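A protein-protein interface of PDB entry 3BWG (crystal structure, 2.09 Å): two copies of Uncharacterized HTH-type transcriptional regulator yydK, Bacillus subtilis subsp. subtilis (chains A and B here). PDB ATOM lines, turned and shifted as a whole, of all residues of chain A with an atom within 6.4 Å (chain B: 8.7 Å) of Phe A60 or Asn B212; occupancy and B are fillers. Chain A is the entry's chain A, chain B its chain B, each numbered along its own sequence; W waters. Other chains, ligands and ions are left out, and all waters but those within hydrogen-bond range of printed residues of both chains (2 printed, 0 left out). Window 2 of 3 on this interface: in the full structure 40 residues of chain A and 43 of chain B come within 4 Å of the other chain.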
ATOM      1  N   GLN A  25       0.274  31.402 -14.217  1.00  0.00           N
ATOM      2  CA  GLN A  25      -0.253  30.046 -14.390  1.00  0.00           C
ATOM      3  C   GLN A  25      -1.022  29.574 -13.161  1.00  0.00           C
ATOM      4  O   GLN A  25      -0.565  29.748 -12.045  1.00  0.00           O
ATOM      5  CB  GLN A  25       0.849  29.053 -14.686  1.00  0.00           C
ATOM      6  CG  GLN A  25       0.282  27.667 -14.892  1.00  0.00           C
ATOM      7  CD  GLN A  25       0.971  26.920 -15.967  1.00  0.00           C
ATOM      8  OE1 GLN A  25       1.187  27.433 -17.072  1.00  0.00           O
ATOM      9  NE2 GLN A  25       1.352  25.686 -15.658  1.00  0.00           N
ATOM     10  N   GLY A  26      -2.196  28.984 -13.380  1.00  0.00           N
ATOM     11  CA  GLY A  26      -2.955  28.374 -12.300  1.00  0.00           C
ATOM     12  C   GLY A  26      -3.890  29.319 -11.575  1.00  0.00           C
ATOM     13  O   GLY A  26      -4.823  28.894 -10.858  1.00  0.00           O
ATOM     14  N   ASP A  27      -3.679  30.613 -11.719  1.00  0.00           N
ATOM     15  CA  ASP A  27      -4.647  31.435 -11.027  1.00  0.00           C
ATOM     16  C   ASP A  27      -5.990  31.530 -11.800  1.00  0.00           C
ATOM     17  O   ASP A  27      -6.039  31.425 -13.035  1.00  0.00           O
ATOM     18  CB  ASP A  27      -4.073  32.670 -10.273  1.00  0.00           C
ATOM     19  CG  ASP A  27      -3.500  33.724 -11.172  1.00  0.00           C
ATOM     20  OD1 ASP A  27      -3.983  33.844 -12.317  1.00  0.00           O
ATOM     21  OD2 ASP A  27      -2.594  34.455 -10.707  1.00  0.00           O
ATOM     22  N   LEU A  53      -9.059  29.507 -26.631  1.00  0.00           N
ATOM     23  CA  LEU A  53      -7.962  29.862 -25.740  1.00  0.00           C
ATOM     24  C   LEU A  53      -7.232  28.632 -25.186  1.00  0.00           C
ATOM     25  O   LEU A  53      -6.037  28.685 -24.948  1.00  0.00           O
ATOM     26  CB  LEU A  53      -8.446  30.745 -24.587  1.00  0.00           C
ATOM     27  CG  LEU A  53      -8.920  32.174 -24.836  1.00  0.00           C
ATOM     28  CD1 LEU A  53      -9.543  32.632 -23.566  1.00  0.00           C
ATOM     29  CD2 LEU A  53      -7.781  33.101 -25.219  1.00  0.00           C
ATOM     30  N   GLU A  54      -7.974  27.545 -24.974  1.00  0.00           N
ATOM     31  CA  GLU A  54      -7.415  26.312 -24.480  1.00  0.00           C
ATOM     32  C   GLU A  54      -6.583  25.616 -25.580  1.00  0.00           C
ATOM     33  O   GLU A  54      -5.426  25.277 -25.339  1.00  0.00           O
ATOM     34  CB  GLU A  54      -8.503  25.407 -23.918  1.00  0.00           C
ATOM     35  CG  GLU A  54      -7.920  24.228 -23.156  1.00  0.00           C
ATOM     36  CD  GLU A  54      -8.927  23.449 -22.328  1.00  0.00           C
ATOM     37  OE1 GLU A  54     -10.131  23.411 -22.685  1.00  0.00           O
ATOM     38  OE2 GLU A  54      -8.491  22.863 -21.301  1.00  0.00           O
ATOM     39  N   GLY A  57      -3.347  27.260 -25.747  1.00  0.00           N
ATOM     40  CA  GLY A  57      -2.430  27.258 -24.598  1.00  0.00           C
ATOM     41  C   GLY A  57      -2.525  28.497 -23.713  1.00  0.00           C
ATOM     42  O   GLY A  57      -1.615  28.776 -22.922  1.00  0.00           O
ATOM     43  N   ALA A  58      -3.625  29.234 -23.812  1.00  0.00           N
ATOM     44  CA  ALA A  58      -3.830  30.406 -22.919  1.00  0.00           C
ATOM     45  C   ALA A  58      -4.460  30.057 -21.571  1.00  0.00           C
ATOM     46  O   ALA A  58      -4.243  30.737 -20.554  1.00  0.00           O
ATOM     47  CB  ALA A  58      -4.632  31.490 -23.610  1.00  0.00           C
ATOM     48  N   ILE A  59      -5.254  28.999 -21.577  1.00  0.00           N
ATOM     49  CA  ILE A  59      -5.973  28.559 -20.389  1.00  0.00           C
ATOM     50  C   ILE A  59      -5.937  27.030 -20.298  1.00  0.00           C
ATOM     51  O   ILE A  59      -5.705  26.308 -21.299  1.00  0.00           O
ATOM     52  CB  ILE A  59      -7.477  29.065 -20.383  1.00  0.00           C
ATOM     53  CG1 ILE A  59      -8.335  28.356 -21.449  1.00  0.00           C
ATOM     54  CG2 ILE A  59      -7.568  30.569 -20.520  1.00  0.00           C
ATOM     55  CD1 ILE A  59      -9.827  28.752 -21.451  1.00  0.00           C
ATOM     56  N   PHE A  60      -6.153  26.536 -19.088  1.00  0.00           N
ATOM     57  CA  PHE A  60      -6.581  25.155 -18.932  1.00  0.00           C
ATOM     58  C   PHE A  60      -7.831  25.075 -18.087  1.00  0.00           C
ATOM     59  O   PHE A  60      -8.075  25.938 -17.225  1.00  0.00           O
ATOM     60  CB  PHE A  60      -5.467  24.229 -18.420  1.00  0.00           C
ATOM     61  CG  PHE A  60      -5.054  24.477 -16.977  1.00  0.00           C
ATOM     62  CD1 PHE A  60      -4.096  25.459 -16.666  1.00  0.00           C
ATOM     63  CD2 PHE A  60      -5.543  23.681 -15.944  1.00  0.00           C
ATOM     64  CE1 PHE A  60      -3.669  25.659 -15.335  1.00  0.00           C
ATOM     65  CE2 PHE A  60      -5.118  23.889 -14.617  1.00  0.00           C
ATOM     66  CZ  PHE A  60      -4.179  24.875 -14.325  1.00  0.00           C
ATOM     67  N   GLN A  61      -8.622  24.035 -18.332  1.00  0.00           N
ATOM     68  CA  GLN A  61      -9.919  23.908 -17.679  1.00  0.00           C
ATOM     69  C   GLN A  61      -9.995  22.590 -16.940  1.00  0.00           C
ATOM     70  O   GLN A  61      -9.486  21.578 -17.416  1.00  0.00           O
ATOM     71  CB  GLN A  61     -11.039  24.027 -18.715  1.00  0.00           C
ATOM     72  CG  GLN A  61     -11.175  25.445 -19.299  1.00  0.00           C
ATOM     73  CD  GLN A  61     -12.213  25.545 -20.425  1.00  0.00           C
ATOM     74  OE1 GLN A  61     -11.955  25.138 -21.566  1.00  0.00           O
ATOM     75  NE2 GLN A  61     -13.377  26.101 -20.108  1.00  0.00           N
ATOM     76  N   VAL A  62     -10.594  22.603 -15.752  1.00  0.00           N
ATOM     77  CA  VAL A  62     -10.815  21.351 -15.036  1.00  0.00           C
ATOM     78  C   VAL A  62     -12.248  21.324 -14.546  1.00  0.00           C
ATOM     79  O   VAL A  62     -12.651  22.171 -13.742  1.00  0.00           O
ATOM     80  CB  VAL A  62      -9.693  20.982 -13.936  1.00  0.00           C
ATOM     81  CG1 VAL A  62      -8.692  22.116 -13.633  1.00  0.00           C
ATOM     82  CG2 VAL A  62     -10.287  20.359 -12.651  1.00  0.00           C
ATOM     83  N   GLY A  66     -12.682  24.930 -12.186  1.00  0.00           N
ATOM     84  CA  GLY A  66     -12.697  26.216 -12.834  1.00  0.00           C
ATOM     85  C   GLY A  66     -11.917  26.333 -14.116  1.00  0.00           C
ATOM     86  O   GLY A  66     -11.611  25.345 -14.806  1.00  0.00           O
ATOM     87  N   ILE A  67     -11.635  27.576 -14.466  1.00  0.00           N
ATOM     88  CA  ILE A  67     -10.868  27.857 -15.658  1.00  0.00           C
ATOM     89  C   ILE A  67      -9.715  28.747 -15.201  1.00  0.00           C
ATOM     90  O   ILE A  67      -9.896  29.697 -14.397  1.00  0.00           O
ATOM     91  CB  ILE A  67     -11.773  28.396 -16.848  1.00  0.00           C
ATOM     92  CG1 ILE A  67     -11.508  29.858 -17.193  1.00  0.00           C
ATOM     93  CG2 ILE A  67     -13.296  28.151 -16.588  1.00  0.00           C
ATOM     94  CD1 ILE A  67     -10.494  29.999 -18.252  1.00  0.00           C
ATOM     95  N   PHE A  68      -8.535  28.392 -15.692  1.00  0.00           N
ATOM     96  CA  PHE A  68      -7.262  28.722 -15.072  1.00  0.00           C
ATOM     97  C   PHE A  68      -6.288  29.238 -16.107  1.00  0.00           C
ATOM     98  O   PHE A  68      -6.135  28.640 -17.175  1.00  0.00           O
ATOM     99  CB  PHE A  68      -6.657  27.446 -14.456  1.00  0.00           C
ATOM    100  CG  PHE A  68      -7.482  26.878 -13.360  1.00  0.00           C
ATOM    101  CD1 PHE A  68      -8.281  25.764 -13.574  1.00  0.00           C
ATOM    102  CD2 PHE A  68      -7.507  27.502 -12.099  1.00  0.00           C
ATOM    103  CE1 PHE A  68      -9.097  25.254 -12.515  1.00  0.00           C
ATOM    104  CE2 PHE A  68      -8.323  27.013 -11.072  1.00  0.00           C
ATOM    105  CZ  PHE A  68      -9.106  25.892 -11.289  1.00  0.00           C
ATOM    106  N   VAL A  69      -5.617  30.336 -15.797  1.00  0.00           N
ATOM    107  CA  VAL A  69      -4.673  30.860 -16.747  1.00  0.00           C
ATOM    108  C   VAL A  69      -3.490  29.916 -16.875  1.00  0.00           C
ATOM    109  O   VAL A  69      -3.069  29.269 -15.897  1.00  0.00           O
ATOM    110  CB  VAL A  69      -4.309  32.376 -16.545  1.00  0.00           C
ATOM    111  CG1 VAL A  69      -4.913  32.946 -15.267  1.00  0.00           C
ATOM    112  CG2 VAL A  69      -2.804  32.666 -16.670  1.00  0.00           C
ATOM    113  N   ARG A  70      -3.010  29.826 -18.105  1.00  0.00           N
ATOM    114  CA  ARG A  70      -1.866  29.009 -18.433  1.00  0.00           C
ATOM    115  C   ARG A  70      -0.798  29.904 -18.994  1.00  0.00           C
ATOM    116  O   ARG A  70      -1.053  30.673 -19.903  1.00  0.00           O
ATOM    117  CB  ARG A  70      -2.248  27.893 -19.397  1.00  0.00           C
ATOM    118  CG  ARG A  70      -1.073  27.347 -20.132  1.00  0.00           C
ATOM    119  CD  ARG A  70      -0.957  25.863 -20.092  1.00  0.00           C
ATOM    120  NE  ARG A  70      -1.510  25.190 -21.255  1.00  0.00           N
ATOM    121  CZ  ARG A  70      -0.867  24.379 -22.093  1.00  0.00           C
ATOM    122  NH1 ARG A  70       0.403  24.066 -21.960  1.00  0.00           N
ATOM    123  NH2 ARG A  70      -1.559  23.817 -23.051  1.00  0.00           N
ATOM    124  N   SER A 236      -3.941  18.520 -23.272  1.00  0.00           N
ATOM    125  CA  SER A 236      -4.059  17.259 -22.557  1.00  0.00           C
ATOM    126  C   SER A 236      -4.089  16.025 -23.478  1.00  0.00           C
ATOM    127  O   SER A 236      -3.164  15.192 -23.440  1.00  0.00           O
ATOM    128  CB  SER A 236      -5.243  17.308 -21.586  1.00  0.00           C
ATOM    129  OG  SER A 236      -5.159  18.484 -20.775  1.00  0.00           O
ATOM    130  N   ILE B 148       3.907  12.305  -6.232  1.00  0.00           N
ATOM    131  CA  ILE B 148       2.995  12.022  -7.355  1.00  0.00           C
ATOM    132  C   ILE B 148       3.290  10.628  -7.983  1.00  0.00           C
ATOM    133  O   ILE B 148       2.427   9.777  -8.041  1.00  0.00           O
ATOM    134  CB  ILE B 148       3.072  13.124  -8.441  1.00  0.00           C
ATOM    135  CG1 ILE B 148       2.743  14.496  -7.803  1.00  0.00           C
ATOM    136  CG2 ILE B 148       2.099  12.748  -9.620  1.00  0.00           C
ATOM    137  CD1 ILE B 148       2.783  15.707  -8.764  1.00  0.00           C
ATOM    138  N   LEU B 171      -3.089   7.955 -13.117  1.00  0.00           N
ATOM    139  CA  LEU B 171      -2.997   9.407 -13.221  1.00  0.00           C
ATOM    140  C   LEU B 171      -3.408   9.901 -14.600  1.00  0.00           C
ATOM    141  O   LEU B 171      -3.245   9.205 -15.596  1.00  0.00           O
ATOM    142  CB  LEU B 171      -1.564   9.874 -12.912  1.00  0.00           C
ATOM    143  CG  LEU B 171      -1.163   9.608 -11.462  1.00  0.00           C
ATOM    144  CD1 LEU B 171       0.292   9.922 -11.268  1.00  0.00           C
ATOM    145  CD2 LEU B 171      -2.037  10.400 -10.499  1.00  0.00           C
ATOM    146  N   LYS B 172      -3.895  11.137 -14.648  1.00  0.00           N
ATOM    147  CA  LYS B 172      -4.397  11.706 -15.877  1.00  0.00           C
ATOM    148  C   LYS B 172      -3.415  12.790 -16.313  1.00  0.00           C
ATOM    149  O   LYS B 172      -3.274  13.833 -15.664  1.00  0.00           O
ATOM    150  CB  LYS B 172      -5.826  12.253 -15.675  1.00  0.00           C
ATOM    151  CG  LYS B 172      -6.787  11.262 -14.996  1.00  0.00           C
ATOM    152  CD  LYS B 172      -7.141  10.084 -15.939  1.00  0.00           C
ATOM    153  CE  LYS B 172      -7.414   8.784 -15.150  1.00  0.00           C
ATOM    154  NZ  LYS B 172      -8.493   8.913 -14.115  1.00  0.00           N
ATOM    155  N   ILE B 173      -2.719  12.496 -17.403  1.00  0.00           N
ATOM    156  CA  ILE B 173      -1.660  13.326 -17.947  1.00  0.00           C
ATOM    157  C   ILE B 173      -2.279  14.444 -18.802  1.00  0.00           C
ATOM    158  O   ILE B 173      -3.075  14.186 -19.692  1.00  0.00           O
ATOM    159  CB  ILE B 173      -0.657  12.444 -18.737  1.00  0.00           C
ATOM    160  CG1 ILE B 173      -0.114  11.327 -17.803  1.00  0.00           C
ATOM    161  CG2 ILE B 173       0.426  13.319 -19.462  1.00  0.00           C
ATOM    162  CD1 ILE B 173       1.057  10.430 -18.361  1.00  0.00           C
ATOM    163  N   GLY B 174      -1.938  15.695 -18.508  1.00  0.00           N
ATOM    164  CA  GLY B 174      -2.562  16.813 -19.197  1.00  0.00           C
ATOM    165  C   GLY B 174      -1.536  17.528 -20.062  1.00  0.00           C
ATOM    166  O   GLY B 174      -0.765  16.886 -20.781  1.00  0.00           O
ATOM    167  N   PHE B 175      -1.513  18.860 -19.972  1.00  0.00           N
ATOM    168  CA  PHE B 175      -0.732  19.663 -20.889  1.00  0.00           C
ATOM    169  C   PHE B 175       0.763  19.598 -20.576  1.00  0.00           C
ATOM    170  O   PHE B 175       1.173  19.220 -19.460  1.00  0.00           O
ATOM    171  CB  PHE B 175      -1.251  21.094 -20.901  1.00  0.00           C
ATOM    172  CG  PHE B 175      -1.190  21.786 -19.557  1.00  0.00           C
ATOM    173  CD1 PHE B 175      -0.086  22.547 -19.200  1.00  0.00           C
ATOM    174  CD2 PHE B 175      -2.270  21.710 -18.665  1.00  0.00           C
ATOM    175  CE1 PHE B 175      -0.034  23.213 -17.967  1.00  0.00           C
ATOM    176  CE2 PHE B 175      -2.227  22.375 -17.412  1.00  0.00           C
ATOM    177  CZ  PHE B 175      -1.109  23.104 -17.060  1.00  0.00           C
ATOM    178  N   PHE B 208       5.809  18.190 -18.114  1.00  0.00           N
ATOM    179  CA  PHE B 208       4.508  17.533 -18.247  1.00  0.00           C
ATOM    180  C   PHE B 208       3.692  17.772 -16.977  1.00  0.00           C
ATOM    181  O   PHE B 208       4.235  17.756 -15.862  1.00  0.00           O
ATOM    182  CB  PHE B 208       4.670  16.042 -18.574  1.00  0.00           C
ATOM    183  CG  PHE B 208       5.327  15.792 -19.919  1.00  0.00           C
ATOM    184  CD1 PHE B 208       4.557  15.506 -21.046  1.00  0.00           C
ATOM    185  CD2 PHE B 208       6.728  15.823 -20.052  1.00  0.00           C
ATOM    186  CE1 PHE B 208       5.173  15.270 -22.307  1.00  0.00           C
ATOM    187  CE2 PHE B 208       7.357  15.557 -21.315  1.00  0.00           C
ATOM    188  CZ  PHE B 208       6.566  15.318 -22.433  1.00  0.00           C
ATOM    189  N   HIS B 209       2.406  18.054 -17.160  1.00  0.00           N
ATOM    190  CA  HIS B 209       1.532  18.419 -16.032  1.00  0.00           C
ATOM    191  C   HIS B 209       0.433  17.367 -15.958  1.00  0.00           C
ATOM    192  O   HIS B 209       0.030  16.794 -16.991  1.00  0.00           O
ATOM    193  CB  HIS B 209       0.892  19.829 -16.232  1.00  0.00           C
ATOM    194  CG  HIS B 209       1.890  20.950 -16.350  1.00  0.00           C
ATOM    195  ND1 HIS B 209       2.588  21.212 -17.516  1.00  0.00           N
ATOM    196  CD2 HIS B 209       2.321  21.864 -15.446  1.00  0.00           C
ATOM    197  CE1 HIS B 209       3.402  22.236 -17.325  1.00  0.00           C
ATOM    198  NE2 HIS B 209       3.288  22.626 -16.071  1.00  0.00           N
ATOM    199  N   LEU B 210      -0.087  17.133 -14.755  1.00  0.00           N
ATOM    200  CA  LEU B 210      -1.354  16.418 -14.613  1.00  0.00           C
ATOM    201  C   LEU B 210      -2.514  17.325 -15.103  1.00  0.00           C
ATOM    202  O   LEU B 210      -2.339  18.537 -15.383  1.00  0.00           O
ATOM    203  CB  LEU B 210      -1.573  15.959 -13.172  1.00  0.00           C
ATOM    204  CG  LEU B 210      -0.563  15.027 -12.473  1.00  0.00           C
ATOM    205  CD1 LEU B 210      -0.944  14.899 -11.021  1.00  0.00           C
ATOM    206  CD2 LEU B 210      -0.475  13.627 -13.146  1.00  0.00           C
ATOM    207  N   THR B 211      -3.690  16.758 -15.289  1.00  0.00           N
ATOM    208  CA  THR B 211      -4.811  17.579 -15.809  1.00  0.00           C
ATOM    209  C   THR B 211      -5.182  18.744 -14.873  1.00  0.00           C
ATOM    210  O   THR B 211      -5.757  19.748 -15.335  1.00  0.00           O
ATOM    211  CB  THR B 211      -6.073  16.748 -16.045  1.00  0.00           C
ATOM    212  OG1 THR B 211      -6.330  15.999 -14.865  1.00  0.00           O
ATOM    213  CG2 THR B 211      -5.914  15.819 -17.244  1.00  0.00           C
ATOM    214  N   ASN B 212      -4.850  18.622 -13.576  1.00  0.00           N
ATOM    215  CA  ASN B 212      -5.077  19.714 -12.594  1.00  0.00           C
ATOM    216  C   ASN B 212      -3.997  20.782 -12.631  1.00  0.00           C
ATOM    217  O   ASN B 212      -4.013  21.719 -11.812  1.00  0.00           O
ATOM    218  CB  ASN B 212      -5.249  19.182 -11.165  1.00  0.00           C
ATOM    219  CG  ASN B 212      -4.056  18.345 -10.698  1.00  0.00           C
ATOM    220  OD1 ASN B 212      -2.928  18.522 -11.146  1.00  0.00           O
ATOM    221  ND2 ASN B 212      -4.313  17.422  -9.790  1.00  0.00           N
ATOM    222  N   GLY B 213      -3.047  20.654 -13.570  1.00  0.00           N
ATOM    223  CA  GLY B 213      -2.056  21.696 -13.763  1.00  0.00           C
ATOM    224  C   GLY B 213      -0.782  21.486 -12.960  1.00  0.00           C
ATOM    225  O   GLY B 213       0.188  22.199 -13.141  1.00  0.00           O
ATOM    226  N   GLN B 214      -0.776  20.494 -12.079  1.00  0.00           N
ATOM    227  CA  GLN B 214       0.398  20.138 -11.286  1.00  0.00           C
ATOM    228  C   GLN B 214       1.535  19.437 -12.111  1.00  0.00           C
ATOM    229  O   GLN B 214       1.298  18.356 -12.717  1.00  0.00           O
ATOM    230  CB  GLN B 214      -0.113  19.252 -10.173  1.00  0.00           C
ATOM    231  CG  GLN B 214       0.873  18.899  -9.089  1.00  0.00           C
ATOM    232  CD  GLN B 214       0.215  18.110  -7.921  1.00  0.00           C
ATOM    233  OE1 GLN B 214      -0.998  17.902  -7.902  1.00  0.00           O
ATOM    234  NE2 GLN B 214       1.018  17.678  -6.969  1.00  0.00           N
ATOM    235  N   PRO B 215       2.783  20.023 -12.128  1.00  0.00           N
ATOM    236  CA  PRO B 215       3.851  19.314 -12.859  1.00  0.00           C
ATOM    237  C   PRO B 215       4.109  17.963 -12.217  1.00  0.00           C
ATOM    238  O   PRO B 215       3.964  17.829 -10.997  1.00  0.00           O
ATOM    239  CB  PRO B 215       5.090  20.197 -12.657  1.00  0.00           C
ATOM    240  CG  PRO B 215       4.598  21.517 -12.206  1.00  0.00           C
ATOM    241  CD  PRO B 215       3.282  21.263 -11.494  1.00  0.00           C
ATOM    242  N   PHE B 216       4.497  16.971 -13.024  1.00  0.00           N
ATOM    243  CA  PHE B 216       4.905  15.658 -12.483  1.00  0.00           C
ATOM    244  C   PHE B 216       6.249  15.152 -13.030  1.00  0.00           C
ATOM    245  O   PHE B 216       6.875  14.282 -12.410  1.00  0.00           O
ATOM    246  CB  PHE B 216       3.805  14.575 -12.664  1.00  0.00           C
ATOM    247  CG  PHE B 216       3.595  14.121 -14.102  1.00  0.00           C
ATOM    248  CD1 PHE B 216       4.306  13.038 -14.630  1.00  0.00           C
ATOM    249  CD2 PHE B 216       2.670  14.756 -14.905  1.00  0.00           C
ATOM    250  CE1 PHE B 216       4.128  12.598 -15.937  1.00  0.00           C
ATOM    251  CE2 PHE B 216       2.473  14.331 -16.250  1.00  0.00           C
ATOM    252  CZ  PHE B 216       3.220  13.245 -16.754  1.00  0.00           C
HETATM  253  O   HOH W   1       0.739  24.703 -13.216  1.00  0.00           O
HETATM  254  O   HOH W   2       4.574  24.963 -15.276  1.00  0.00           O
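The backbone NH (N) of Arg A70 sits at hydrogen-bond distance from the backbone carbonyl oxygen (O) of Ala A58, 2.9 Å away.
N of Phe A60 sits at hydrogen-bond distance from O of Phe A68.
N of Thr B211 sits at hydrogen-bond distance from O of Lys B172 (3.0 Å).
N of Gly B174 is in hydrogen-bond range of O of His B209, at 2.7 Å.
O of Phe B175 lies within hydrogen-bond range of N of His B209, 2.9 Å away.
The side-chain amide oxygen of Asn B212 sits at hydrogen-bond distance from the backbone NH of Gln B214 (3.1 Å).
Among the printed residues, merely in contact across the chains: Arg A70 with Phe B175, Ser A236 with Gly B174, Phe A60 with Phe B175, Gln A25 with His B209, Gln A25 with Phe B175, Phe A60 with Asn B212, Ser A236 with Phe B175, Phe A60 with Gly B213, Ser A236 with Ile B173 and Phe A60 with Thr B211.
Printed residues of chain B within 4 Å of Gln A25: Phe B175 and His B209.
Glu A54 touches none of the printed residues of chain B.
Gly A57 touches none of the printed residues of chain B.
Of the printed residues of chain B, Arg A70 touches Phe B175.
Of the printed residues of chain A, Phe B175 touches Gln A25, Phe A60, Arg A70 and Ser A236.
Of the printed residues of chain A, Asn B212 touches Phe A60.
Of the printed residues of chain A, Gly B213 touches Phe A60 (3.9 Å).
The nearest printed residue of chain B that does not touch Phe A60 is Gln B214 (6.0 Å).
The nearest printed residue of chain B that does not touch Gln A25 is Gly B213 (4.5 Å).
Printed residues of chain B that touch a printed residue of chain A: Ile B173, Gly B174, Phe B175, His B209, Thr B211, Asn B212 and Gly B213.
Hydrophobic or aromatic side chains of chain B within 4 Å of the printed part of chain A: Phe B175 and His B209.
Among the printed residues, 10 pairs touch across the chains.
Among the printed residues, no Asp or Glu carboxylate lies within 4 Å of a Lys or Arg side-chain nitrogen of the other chain.
No position is printed for both chains.
Of the 10 pairs that touch across the chains among the printed residues, none has its exchanged pair printed and touching as well.
Water W1 lies within hydrogen-bond range of the backbone carbonyl oxygen of Gly B213 and the side-chain amide nitrogen of Gln A25.
Water W2 lies within hydrogen-bond range of NE2 of His B209 (2.8 Å) and NE2 of Gln A25 (3.3 Å).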
